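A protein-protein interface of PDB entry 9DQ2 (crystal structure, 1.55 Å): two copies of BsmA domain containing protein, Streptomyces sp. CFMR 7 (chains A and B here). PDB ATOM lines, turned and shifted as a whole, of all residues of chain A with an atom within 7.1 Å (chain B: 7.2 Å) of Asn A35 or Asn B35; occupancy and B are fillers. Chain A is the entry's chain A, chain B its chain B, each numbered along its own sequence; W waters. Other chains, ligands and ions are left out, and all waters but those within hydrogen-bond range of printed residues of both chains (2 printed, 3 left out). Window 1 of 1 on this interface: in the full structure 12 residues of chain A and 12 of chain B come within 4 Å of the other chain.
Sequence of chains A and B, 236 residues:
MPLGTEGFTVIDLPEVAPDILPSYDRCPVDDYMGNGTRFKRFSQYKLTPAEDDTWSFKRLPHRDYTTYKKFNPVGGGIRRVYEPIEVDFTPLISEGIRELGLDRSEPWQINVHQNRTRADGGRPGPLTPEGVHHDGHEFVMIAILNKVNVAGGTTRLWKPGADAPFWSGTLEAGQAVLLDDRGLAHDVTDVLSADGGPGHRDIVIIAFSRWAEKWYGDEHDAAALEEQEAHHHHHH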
ATOM      1  N   VAL A  29      11.189   5.277   1.750  1.00  0.00           N
ATOM      2  CA  VAL A  29      11.919   4.598   0.677  1.00  0.00           C
ATOM      3  C   VAL A  29      11.118   4.673  -0.625  1.00  0.00           C
ATOM      4  O   VAL A  29       9.874   4.631  -0.637  1.00  0.00           O
ATOM      5  CB  VAL A  29      12.254   3.142   1.054  1.00  0.00           C
ATOM      6  CG1 VAL A  29      10.999   2.255   1.048  1.00  0.00           C
ATOM      7  CG2 VAL A  29      13.308   2.573   0.127  1.00  0.00           C
ATOM      8  N   ASP A  30      11.845   4.846  -1.726  1.00  0.00           N
ATOM      9  CA  ASP A  30      11.277   4.796  -3.077  1.00  0.00           C
ATOM     10  C   ASP A  30      11.106   3.333  -3.457  1.00  0.00           C
ATOM     11  O   ASP A  30      12.101   2.613  -3.605  1.00  0.00           O
ATOM     12  CB  ASP A  30      12.226   5.515  -4.030  1.00  0.00           C
ATOM     13  CG  ASP A  30      11.701   5.645  -5.464  1.00  0.00           C
ATOM     14  OD1 ASP A  30      10.734   4.946  -5.874  1.00  0.00           O
ATOM     15  OD2 ASP A  30      12.304   6.490  -6.173  1.00  0.00           O
ATOM     16  N   ASP A  31       9.851   2.869  -3.573  1.00  0.00           N
ATOM     17  CA  ASP A  31       9.626   1.455  -3.840  1.00  0.00           C
ATOM     18  C   ASP A  31       9.907   1.069  -5.282  1.00  0.00           C
ATOM     19  O   ASP A  31       9.905  -0.129  -5.602  1.00  0.00           O
ATOM     20  CB  ASP A  31       8.182   1.060  -3.512  1.00  0.00           C
ATOM     21  CG  ASP A  31       7.886   1.139  -2.028  1.00  0.00           C
ATOM     22  OD1 ASP A  31       8.720   0.651  -1.236  1.00  0.00           O
ATOM     23  OD2 ASP A  31       6.833   1.714  -1.663  1.00  0.00           O
ATOM     24  N   TYR A  32      10.179   2.030  -6.153  1.00  0.00           N
ATOM     25  CA  TYR A  32      10.195   1.762  -7.579  1.00  0.00           C
ATOM     26  C   TYR A  32      11.539   1.934  -8.238  1.00  0.00           C
ATOM     27  O   TYR A  32      11.733   1.424  -9.355  1.00  0.00           O
ATOM     28  CB  TYR A  32       9.220   2.689  -8.295  1.00  0.00           C
ATOM     29  CG  TYR A  32       7.849   2.655  -7.689  1.00  0.00           C
ATOM     30  CD1 TYR A  32       6.912   1.690  -8.082  1.00  0.00           C
ATOM     31  CD2 TYR A  32       7.476   3.600  -6.752  1.00  0.00           C
ATOM     32  CE1 TYR A  32       5.620   1.679  -7.555  1.00  0.00           C
ATOM     33  CE2 TYR A  32       6.182   3.599  -6.204  1.00  0.00           C
ATOM     34  CZ  TYR A  32       5.255   2.633  -6.622  1.00  0.00           C
ATOM     35  OH  TYR A  32       3.981   2.629  -6.074  1.00  0.00           O
ATOM     36  N   MET A  33      12.430   2.699  -7.633  1.00  0.00           N
ATOM     37  CA  MET A  33      13.731   2.971  -8.205  1.00  0.00           C
ATOM     38  C   MET A  33      14.784   2.939  -7.120  1.00  0.00           C
ATOM     39  O   MET A  33      14.512   3.249  -5.955  1.00  0.00           O
ATOM     40  CB  MET A  33      13.763   4.321  -8.918  1.00  0.00           C
ATOM     41  CG  MET A  33      12.893   4.328 -10.137  1.00  0.00           C
ATOM     42  SD  MET A  33      13.194   5.736 -11.187  1.00  0.00           S
ATOM     43  CE  MET A  33      14.803   5.379 -11.887  1.00  0.00           C
ATOM     44  N   GLY A  34      15.966   2.538  -7.543  1.00  0.00           N
ATOM     45  CA  GLY A  34      17.161   2.576  -6.719  1.00  0.00           C
ATOM     46  C   GLY A  34      17.361   1.379  -5.831  1.00  0.00           C
ATOM     47  O   GLY A  34      18.339   1.344  -5.080  1.00  0.00           O
ATOM     48  N   ASN A  35      16.479   0.383  -5.897  1.00  0.00           N
ATOM     49  CA  ASN A  35      16.682  -0.882  -5.184  1.00  0.00           C
ATOM     50  C   ASN A  35      17.049  -0.675  -3.711  1.00  0.00           C
ATOM     51  O   ASN A  35      17.985  -1.285  -3.167  1.00  0.00           O
ATOM     52  CB  ASN A  35      17.693  -1.745  -5.932  1.00  0.00           C
ATOM     53  CG  ASN A  35      17.101  -2.296  -7.193  1.00  0.00           C
ATOM     54  OD1 ASN A  35      16.331  -3.258  -7.128  1.00  0.00           O
ATOM     55  ND2 ASN A  35      17.412  -1.693  -8.334  1.00  0.00           N
ATOM     56  N   GLY A  36      16.253   0.173  -3.059  1.00  0.00           N
ATOM     57  CA  GLY A  36      16.367   0.393  -1.637  1.00  0.00           C
ATOM     58  C   GLY A  36      17.347   1.465  -1.229  1.00  0.00           C
ATOM     59  O   GLY A  36      17.464   1.725  -0.019  1.00  0.00           O
ATOM     60  N   THR A  37      18.091   2.046  -2.178  1.00  0.00           N
ATOM     61  CA  THR A  37      19.063   3.110  -1.871  1.00  0.00           C
ATOM     62  C   THR A  37      18.470   4.508  -1.928  1.00  0.00           C
ATOM     63  O   THR A  37      19.185   5.469  -1.598  1.00  0.00           O
ATOM     64  CB  THR A  37      20.270   3.079  -2.816  1.00  0.00           C
ATOM     65  OG1 THR A  37      19.859   3.410  -4.141  1.00  0.00           O
ATOM     66  CG2 THR A  37      20.956   1.669  -2.827  1.00  0.00           C
ATOM     67  N   ARG A  38      17.226   4.646  -2.371  1.00  0.00           N
ATOM     68  CA  ARG A  38      16.617   5.953  -2.642  1.00  0.00           C
ATOM     69  C   ARG A  38      15.369   6.168  -1.789  1.00  0.00           C
ATOM     70  O   ARG A  38      14.598   5.228  -1.534  1.00  0.00           O
ATOM     71  CB  ARG A  38      16.260   6.050  -4.136  1.00  0.00           C
ATOM     72  CG  ARG A  38      15.834   7.429  -4.563  1.00  0.00           C
ATOM     73  CD  ARG A  38      15.585   7.445  -6.068  1.00  0.00           C
ATOM     74  NE  ARG A  38      16.825   7.186  -6.781  1.00  0.00           N
ATOM     75  CZ  ARG A  38      16.955   7.404  -8.081  1.00  0.00           C
ATOM     76  NH1 ARG A  38      15.925   7.825  -8.799  1.00  0.00           N
ATOM     77  NH2 ARG A  38      18.140   7.192  -8.669  1.00  0.00           N
ATOM     78  N   VAL A  74      13.470   2.171 -16.849  1.00  0.00           N
ATOM     79  CA  VAL A  74      13.414   1.382 -15.617  1.00  0.00           C
ATOM     80  C   VAL A  74      12.318   1.842 -14.664  1.00  0.00           C
ATOM     81  O   VAL A  74      11.927   1.064 -13.776  1.00  0.00           O
ATOM     82  CB  VAL A  74      14.770   1.377 -14.872  1.00  0.00           C
ATOM     83  CG1 VAL A  74      15.835   0.678 -15.714  1.00  0.00           C
ATOM     84  CG2 VAL A  74      15.208   2.785 -14.520  1.00  0.00           C
ATOM     85  N   ARG A 123      28.358  -0.645  -1.565  1.00  0.00           N
ATOM     86  CA  ARG A 123      27.060  -0.432  -2.213  1.00  0.00           C
ATOM     87  C   ARG A 123      26.909   1.026  -2.619  1.00  0.00           C
ATOM     88  O   ARG A 123      26.386   1.846  -1.845  1.00  0.00           O
ATOM     89  CB  ARG A 123      25.891  -0.837  -1.332  1.00  0.00           C
ATOM     90  CG  ARG A 123      24.511  -0.796  -2.065  1.00  0.00           C
ATOM     91  CD  ARG A 123      24.276  -2.023  -2.896  1.00  0.00           C
ATOM     92  NE  ARG A 123      23.061  -1.892  -3.700  1.00  0.00           N
ATOM     93  CZ  ARG A 123      21.841  -2.198  -3.282  1.00  0.00           C
ATOM     94  NH1 ARG A 123      21.621  -2.736  -2.091  1.00  0.00           N
ATOM     95  NH2 ARG A 123      20.809  -1.947  -4.086  1.00  0.00           N
ATOM     96  N   PRO A 126      22.897   4.426  -6.860  1.00  0.00           N
ATOM     97  CA  PRO A 126      22.743   4.816  -8.261  1.00  0.00           C
ATOM     98  C   PRO A 126      21.864   6.041  -8.385  1.00  0.00           C
ATOM     99  O   PRO A 126      20.848   6.184  -7.695  1.00  0.00           O
ATOM    100  CB  PRO A 126      22.078   3.594  -8.916  1.00  0.00           C
ATOM    101  CG  PRO A 126      22.299   2.473  -7.942  1.00  0.00           C
ATOM    102  CD  PRO A 126      22.284   3.117  -6.583  1.00  0.00           C
ATOM    103  N   PRO A 129      19.935   5.220 -13.144  1.00  0.00           N
ATOM    104  CA  PRO A 129      19.840   3.882 -13.734  1.00  0.00           C
ATOM    105  C   PRO A 129      19.236   3.889 -15.125  1.00  0.00           C
ATOM    106  O   PRO A 129      19.418   2.907 -15.861  1.00  0.00           O
ATOM    107  CB  PRO A 129      18.969   3.120 -12.729  1.00  0.00           C
ATOM    108  CG  PRO A 129      18.203   4.182 -12.002  1.00  0.00           C
ATOM    109  CD  PRO A 129      19.120   5.371 -11.926  1.00  0.00           C
ATOM    110  N   VAL B  29      14.423 -11.945  -1.063  1.00  0.00           N
ATOM    111  CA  VAL B  29      14.347 -10.835  -2.016  1.00  0.00           C
ATOM    112  C   VAL B  29      15.726 -10.495  -2.558  1.00  0.00           C
ATOM    113  O   VAL B  29      16.755 -10.588  -1.868  1.00  0.00           O
ATOM    114  CB  VAL B  29      13.664  -9.602  -1.406  1.00  0.00           C
ATOM    115  CG1 VAL B  29      14.518  -8.968  -0.311  1.00  0.00           C
ATOM    116  CG2 VAL B  29      13.328  -8.560  -2.494  1.00  0.00           C
ATOM    117  N   ASP B  30      15.754 -10.149  -3.847  1.00  0.00           N
ATOM    118  CA  ASP B  30      16.950  -9.667  -4.535  1.00  0.00           C
ATOM    119  C   ASP B  30      17.121  -8.205  -4.165  1.00  0.00           C
ATOM    120  O   ASP B  30      16.299  -7.370  -4.548  1.00  0.00           O
ATOM    121  CB  ASP B  30      16.790  -9.842  -6.049  1.00  0.00           C
ATOM    122  CG  ASP B  30      18.049  -9.502  -6.836  1.00  0.00           C
ATOM    123  OD1 ASP B  30      18.958  -8.786  -6.332  1.00  0.00           O
ATOM    124  OD2 ASP B  30      18.146  -9.973  -7.984  1.00  0.00           O
ATOM    125  N   ASP B  31      18.140  -7.890  -3.359  1.00  0.00           N
ATOM    126  CA  ASP B  31      18.275  -6.512  -2.897  1.00  0.00           C
ATOM    127  C   ASP B  31      18.835  -5.583  -3.964  1.00  0.00           C
ATOM    128  O   ASP B  31      18.855  -4.357  -3.748  1.00  0.00           O
ATOM    129  CB  ASP B  31      19.221  -6.444  -1.680  1.00  0.00           C
ATOM    130  CG  ASP B  31      18.621  -7.054  -0.417  1.00  0.00           C
ATOM    131  OD1 ASP B  31      17.390  -6.935  -0.198  1.00  0.00           O
ATOM    132  OD2 ASP B  31      19.404  -7.641   0.362  1.00  0.00           O
ATOM    133  N   TYR B  32      19.228  -6.104  -5.124  1.00  0.00           N
ATOM    134  CA  TYR B  32      19.996  -5.327  -6.080  1.00  0.00           C
ATOM    135  C   TYR B  32      19.275  -5.049  -7.374  1.00  0.00           C
ATOM    136  O   TYR B  32      19.677  -4.126  -8.104  1.00  0.00           O
ATOM    137  CB  TYR B  32      21.299  -6.048  -6.421  1.00  0.00           C
ATOM    138  CG  TYR B  32      22.110  -6.395  -5.206  1.00  0.00           C
ATOM    139  CD1 TYR B  32      23.005  -5.485  -4.668  1.00  0.00           C
ATOM    140  CD2 TYR B  32      21.999  -7.649  -4.631  1.00  0.00           C
ATOM    141  CE1 TYR B  32      23.761  -5.808  -3.537  1.00  0.00           C
ATOM    142  CE2 TYR B  32      22.748  -7.996  -3.491  1.00  0.00           C
ATOM    143  CZ  TYR B  32      23.626  -7.068  -2.963  1.00  0.00           C
ATOM    144  OH  TYR B  32      24.366  -7.429  -1.845  1.00  0.00           O
ATOM    145  N   MET B  33      18.294  -5.870  -7.714  1.00  0.00           N
ATOM    146  CA  MET B  33      17.586  -5.820  -8.990  1.00  0.00           C
ATOM    147  C   MET B  33      16.102  -5.991  -8.731  1.00  0.00           C
ATOM    148  O   MET B  33      15.711  -6.784  -7.863  1.00  0.00           O
ATOM    149  CB  MET B  33      18.032  -6.948  -9.949  1.00  0.00           C
ATOM    150  CG  MET B  33      19.463  -6.841 -10.437  1.00  0.00           C
ATOM    151  SD  MET B  33      19.697  -5.495 -11.612  1.00  0.00           S
ATOM    152  CE  MET B  33      19.078  -6.194 -13.144  1.00  0.00           C
ATOM    153  N   GLY B  34      15.292  -5.314  -9.512  1.00  0.00           N
ATOM    154  CA  GLY B  34      13.861  -5.575  -9.540  1.00  0.00           C
ATOM    155  C   GLY B  34      13.032  -4.756  -8.586  1.00  0.00           C
ATOM    156  O   GLY B  34      11.811  -4.900  -8.578  1.00  0.00           O
ATOM    157  N   ASN B  35      13.668  -3.916  -7.766  1.00  0.00           N
ATOM    158  CA  ASN B  35      12.965  -3.006  -6.851  1.00  0.00           C
ATOM    159  C   ASN B  35      11.869  -3.717  -6.051  1.00  0.00           C
ATOM    160  O   ASN B  35      10.713  -3.273  -5.961  1.00  0.00           O
ATOM    161  CB  ASN B  35      12.433  -1.772  -7.611  1.00  0.00           C
ATOM    162  CG  ASN B  35      13.554  -0.859  -8.017  1.00  0.00           C
ATOM    163  OD1 ASN B  35      14.069  -0.144  -7.167  1.00  0.00           O
ATOM    164  ND2 ASN B  35      13.999  -0.950  -9.261  1.00  0.00           N
ATOM    165  N   GLY B  36      12.269  -4.850  -5.427  1.00  0.00           N
ATOM    166  CA  GLY B  36      11.412  -5.616  -4.556  1.00  0.00           C
ATOM    167  C   GLY B  36      10.502  -6.621  -5.232  1.00  0.00           C
ATOM    168  O   GLY B  36       9.772  -7.330  -4.524  1.00  0.00           O
ATOM    169  N   THR B  37      10.514  -6.714  -6.573  1.00  0.00           N
ATOM    170  CA  THR B  37       9.675  -7.680  -7.277  1.00  0.00           C
ATOM    171  C   THR B  37      10.382  -8.996  -7.546  1.00  0.00           C
ATOM    172  O   THR B  37       9.735  -9.929  -8.053  1.00  0.00           O
ATOM    173  CB  THR B  37       9.185  -7.116  -8.626  1.00  0.00           C
ATOM    174  OG1 THR B  37      10.284  -6.961  -9.515  1.00  0.00           O
ATOM    175  CG2 THR B  37       8.466  -5.781  -8.455  1.00  0.00           C
ATOM    176  N   ARG B  38      11.679  -9.096  -7.234  1.00  0.00           N
ATOM    177  CA  ARG B  38      12.491 -10.247  -7.624  1.00  0.00           C
ATOM    178  C   ARG B  38      13.055 -10.941  -6.392  1.00  0.00           C
ATOM    179  O   ARG B  38      13.429 -10.284  -5.414  1.00  0.00           O
ATOM    180  CB  ARG B  38      13.621  -9.820  -8.551  1.00  0.00           C
ATOM    181  CG  ARG B  38      14.354 -10.999  -9.146  1.00  0.00           C
ATOM    182  CD  ARG B  38      15.415 -10.518 -10.139  1.00  0.00           C
ATOM    183  NE  ARG B  38      14.764  -9.818 -11.241  1.00  0.00           N
ATOM    184  CZ  ARG B  38      15.401  -9.502 -12.359  1.00  0.00           C
ATOM    185  NH1 ARG B  38      16.689  -9.762 -12.505  1.00  0.00           N
ATOM    186  NH2 ARG B  38      14.726  -8.918 -13.355  1.00  0.00           N
ATOM    187  N   VAL B  74      22.511  -1.815 -14.841  1.00  0.00           N
ATOM    188  CA  VAL B  74      21.704  -1.585 -13.642  1.00  0.00           C
ATOM    189  C   VAL B  74      22.173  -2.453 -12.480  1.00  0.00           C
ATOM    190  O   VAL B  74      21.926  -2.128 -11.308  1.00  0.00           O
ATOM    191  CB  VAL B  74      20.218  -1.852 -13.962  1.00  0.00           C
ATOM    192  CG1 VAL B  74      19.359  -1.701 -12.761  1.00  0.00           C
ATOM    193  CG2 VAL B  74      19.733  -0.921 -15.074  1.00  0.00           C
ATOM    194  N   ARG B 123       1.409  -3.254 -10.695  1.00  0.00           N
ATOM    195  CA  ARG B 123       2.861  -3.338 -10.495  1.00  0.00           C
ATOM    196  C   ARG B 123       3.395  -4.536 -11.258  1.00  0.00           C
ATOM    197  O   ARG B 123       3.483  -5.643 -10.720  1.00  0.00           O
ATOM    198  CB  ARG B 123       3.258  -3.422  -9.023  1.00  0.00           C
ATOM    199  CG  ARG B 123       4.803  -3.357  -8.804  1.00  0.00           C
ATOM    200  CD  ARG B 123       5.330  -1.960  -8.989  1.00  0.00           C
ATOM    201  NE  ARG B 123       6.795  -1.957  -8.970  1.00  0.00           N
ATOM    202  CZ  ARG B 123       7.559  -1.943  -7.886  1.00  0.00           C
ATOM    203  NH1 ARG B 123       7.037  -1.870  -6.665  1.00  0.00           N
ATOM    204  NH2 ARG B 123       8.890  -1.971  -8.039  1.00  0.00           N
ATOM    205  N   PRO B 126       9.402  -6.500 -13.596  1.00  0.00           N
ATOM    206  CA  PRO B 126      10.358  -6.348 -14.696  1.00  0.00           C
ATOM    207  C   PRO B 126      11.313  -7.532 -14.747  1.00  0.00           C
ATOM    208  O   PRO B 126      11.801  -8.037 -13.721  1.00  0.00           O
ATOM    209  CB  PRO B 126      11.102  -5.038 -14.386  1.00  0.00           C
ATOM    210  CG  PRO B 126      10.380  -4.421 -13.269  1.00  0.00           C
ATOM    211  CD  PRO B 126       9.571  -5.478 -12.550  1.00  0.00           C
ATOM    212  N   PRO B 129      15.437  -5.226 -16.824  1.00  0.00           N
ATOM    213  CA  PRO B 129      15.717  -3.792 -16.697  1.00  0.00           C
ATOM    214  C   PRO B 129      16.993  -3.345 -17.409  1.00  0.00           C
ATOM    215  O   PRO B 129      17.115  -2.147 -17.707  1.00  0.00           O
ATOM    216  CB  PRO B 129      15.809  -3.585 -15.176  1.00  0.00           C
ATOM    217  CG  PRO B 129      16.075  -4.930 -14.594  1.00  0.00           C
ATOM    218  CD  PRO B 129      15.464  -5.946 -15.535  1.00  0.00           C
HETATM  219  O   HOH W   1      18.888  -2.424  -0.863  1.00  0.00           O
HETATM  220  O   HOH W   2       8.501  -2.806  -4.310  1.00  0.00           O
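Tyr A32 touches Asn B35, and with the chains exchanged Asn A35 touches Tyr B32.
Gly A34 touches Asn B35, and with the chains exchanged Asn A35 touches Gly B34.
Asn B35 touches its own counterpart, Asn A35.
Val A74 touches Pro B129, and with the chains exchanged Pro A129 touches Val B74.
Positions printed for both chains: 29, 30, 31, 32, 33, 34, 35, 36, 37, 38, 74, 123, 126 and 129.
Among the printed residues, merely in contact across the chains: Tyr A32 with Arg B123 (3.7 Å), Val A74 with Pro B129 (3.7 Å), Arg A123 with Tyr B32 (3.7 Å) and Pro A129 with Val B74 (3.9 Å).
NH2 of Arg B123 sits at hydrogen-bond distance from O of Asp A31 (3.2 Å).
ND2 of Asn B35 sits close to O of Tyr A32.
N of Met A33 sits close to OD1 of Asn B35 (3.3 Å).
OD1 of Asn B35 is in hydrogen-bond range of N of Gly A34 (3.3 Å).
The backbone carbonyl oxygen of Tyr B32 sits close to the side-chain amide nitrogen of Asn A35 (3.3 Å).
OD1 of Asn A35 sits close to N of Met B33 (3.3 Å).
The backbone NH (N) of Gly B34 sits at hydrogen-bond distance from the side-chain amide oxygen (OD1) of Asn A35 (3.3 Å).
The backbone NH (N) of Asn A35 is in hydrogen-bond range of the side-chain amide oxygen (OD1) of Asn B35, at 2.8 Å.
O of Asp B31 is in hydrogen-bond range of NH2 of Arg A123, 3.1 Å away.
O of Asn B35 lies close to O of Asp A31.
O of Asn A35 sits close to O of Asp B31 (3.2 Å).
The backbone NH (N) of Tyr A32 is in hydrogen-bond range of the side-chain carboxylate (OD1) of Asp A30.
O of Gly A34 lies within hydrogen-bond range of OG1 of Thr A37, 2.7 Å away.
OD1 of Asp B30 is in hydrogen-bond range of N of Tyr B32.
N of Met B33 sits at hydrogen-bond distance from OD1 of Asp B30, 3.3 Å away.
The backbone carbonyl oxygen (O) of Gly B34 is in hydrogen-bond range of the side-chain hydroxyl (OG1) of Thr B37, 2.7 Å away.
O of Asn B35 lies within hydrogen-bond range of NH2 of Arg B123.
Water W1 lies within hydrogen-bond range of the backbone carbonyl oxygen of Asn A35 (2.7 Å), the guanidinium group of Arg A123 (3.0 Å) and the backbone carbonyl oxygen of Asp B31 (3.5 Å).
Water W2 lies within hydrogen-bond range of O of Asn B35 (2.8 Å), NH1 of Arg B123 (2.9 Å) and O of Asp A31 (3.3 Å).
Printed residues of chain B within 4 Å of Asp A31: Asn B35 and Arg B123.
Of the printed residues of chain B, Met A33 touches Asn B35 (3.2 Å).
Of the printed residues of chain B, Asn A35 touches Asp B31 (3.2 Å), Tyr B32 (3.3 Å), Met B33 (3.2 Å), Gly B34 (3.3 Å) and Asn B35 (2.8 Å).
Arg A38 touches none of the printed residues of chain B.
Printed residues of chain A within 4 Å of Asn B35: Asp A31, Tyr A32, Met A33, Gly A34 and Asn A35.
Of the printed residues of chain A, Arg B123 touches Asp A31 and Tyr A32.
The nearest printed residue of chain B that does not touch Asn A35 is Gly B36 (4.7 Å).
The nearest printed residue of chain A that does not touch Asn B35 is Gly A36 (4.7 Å).
The nearest printed residue of chain B that does not touch Val A74 is Val B74 (4.3 Å).
Of the 14 printed residues of chain A, 8 touch a printed residue of chain B.
Hydrophobic or aromatic side chains of chain A that line the printed part of chain B: Tyr A32 and Val A74.
Printed residues of chain B that touch a printed residue of chain A: Asp B31, Tyr B32, Met B33, Gly B34, Asn B35, Val B74, Arg B123 and Pro B129.
Hydrophobic or aromatic side chains of chain B that line the printed part of chain A: Tyr B32 and Val B74.
Among the printed residues, 15 pairs touch across the chains.
Among the printed residues, no Asp or Glu carboxylate lies within 4 Å of a Lys or Arg side-chain nitrogen of the other chain.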
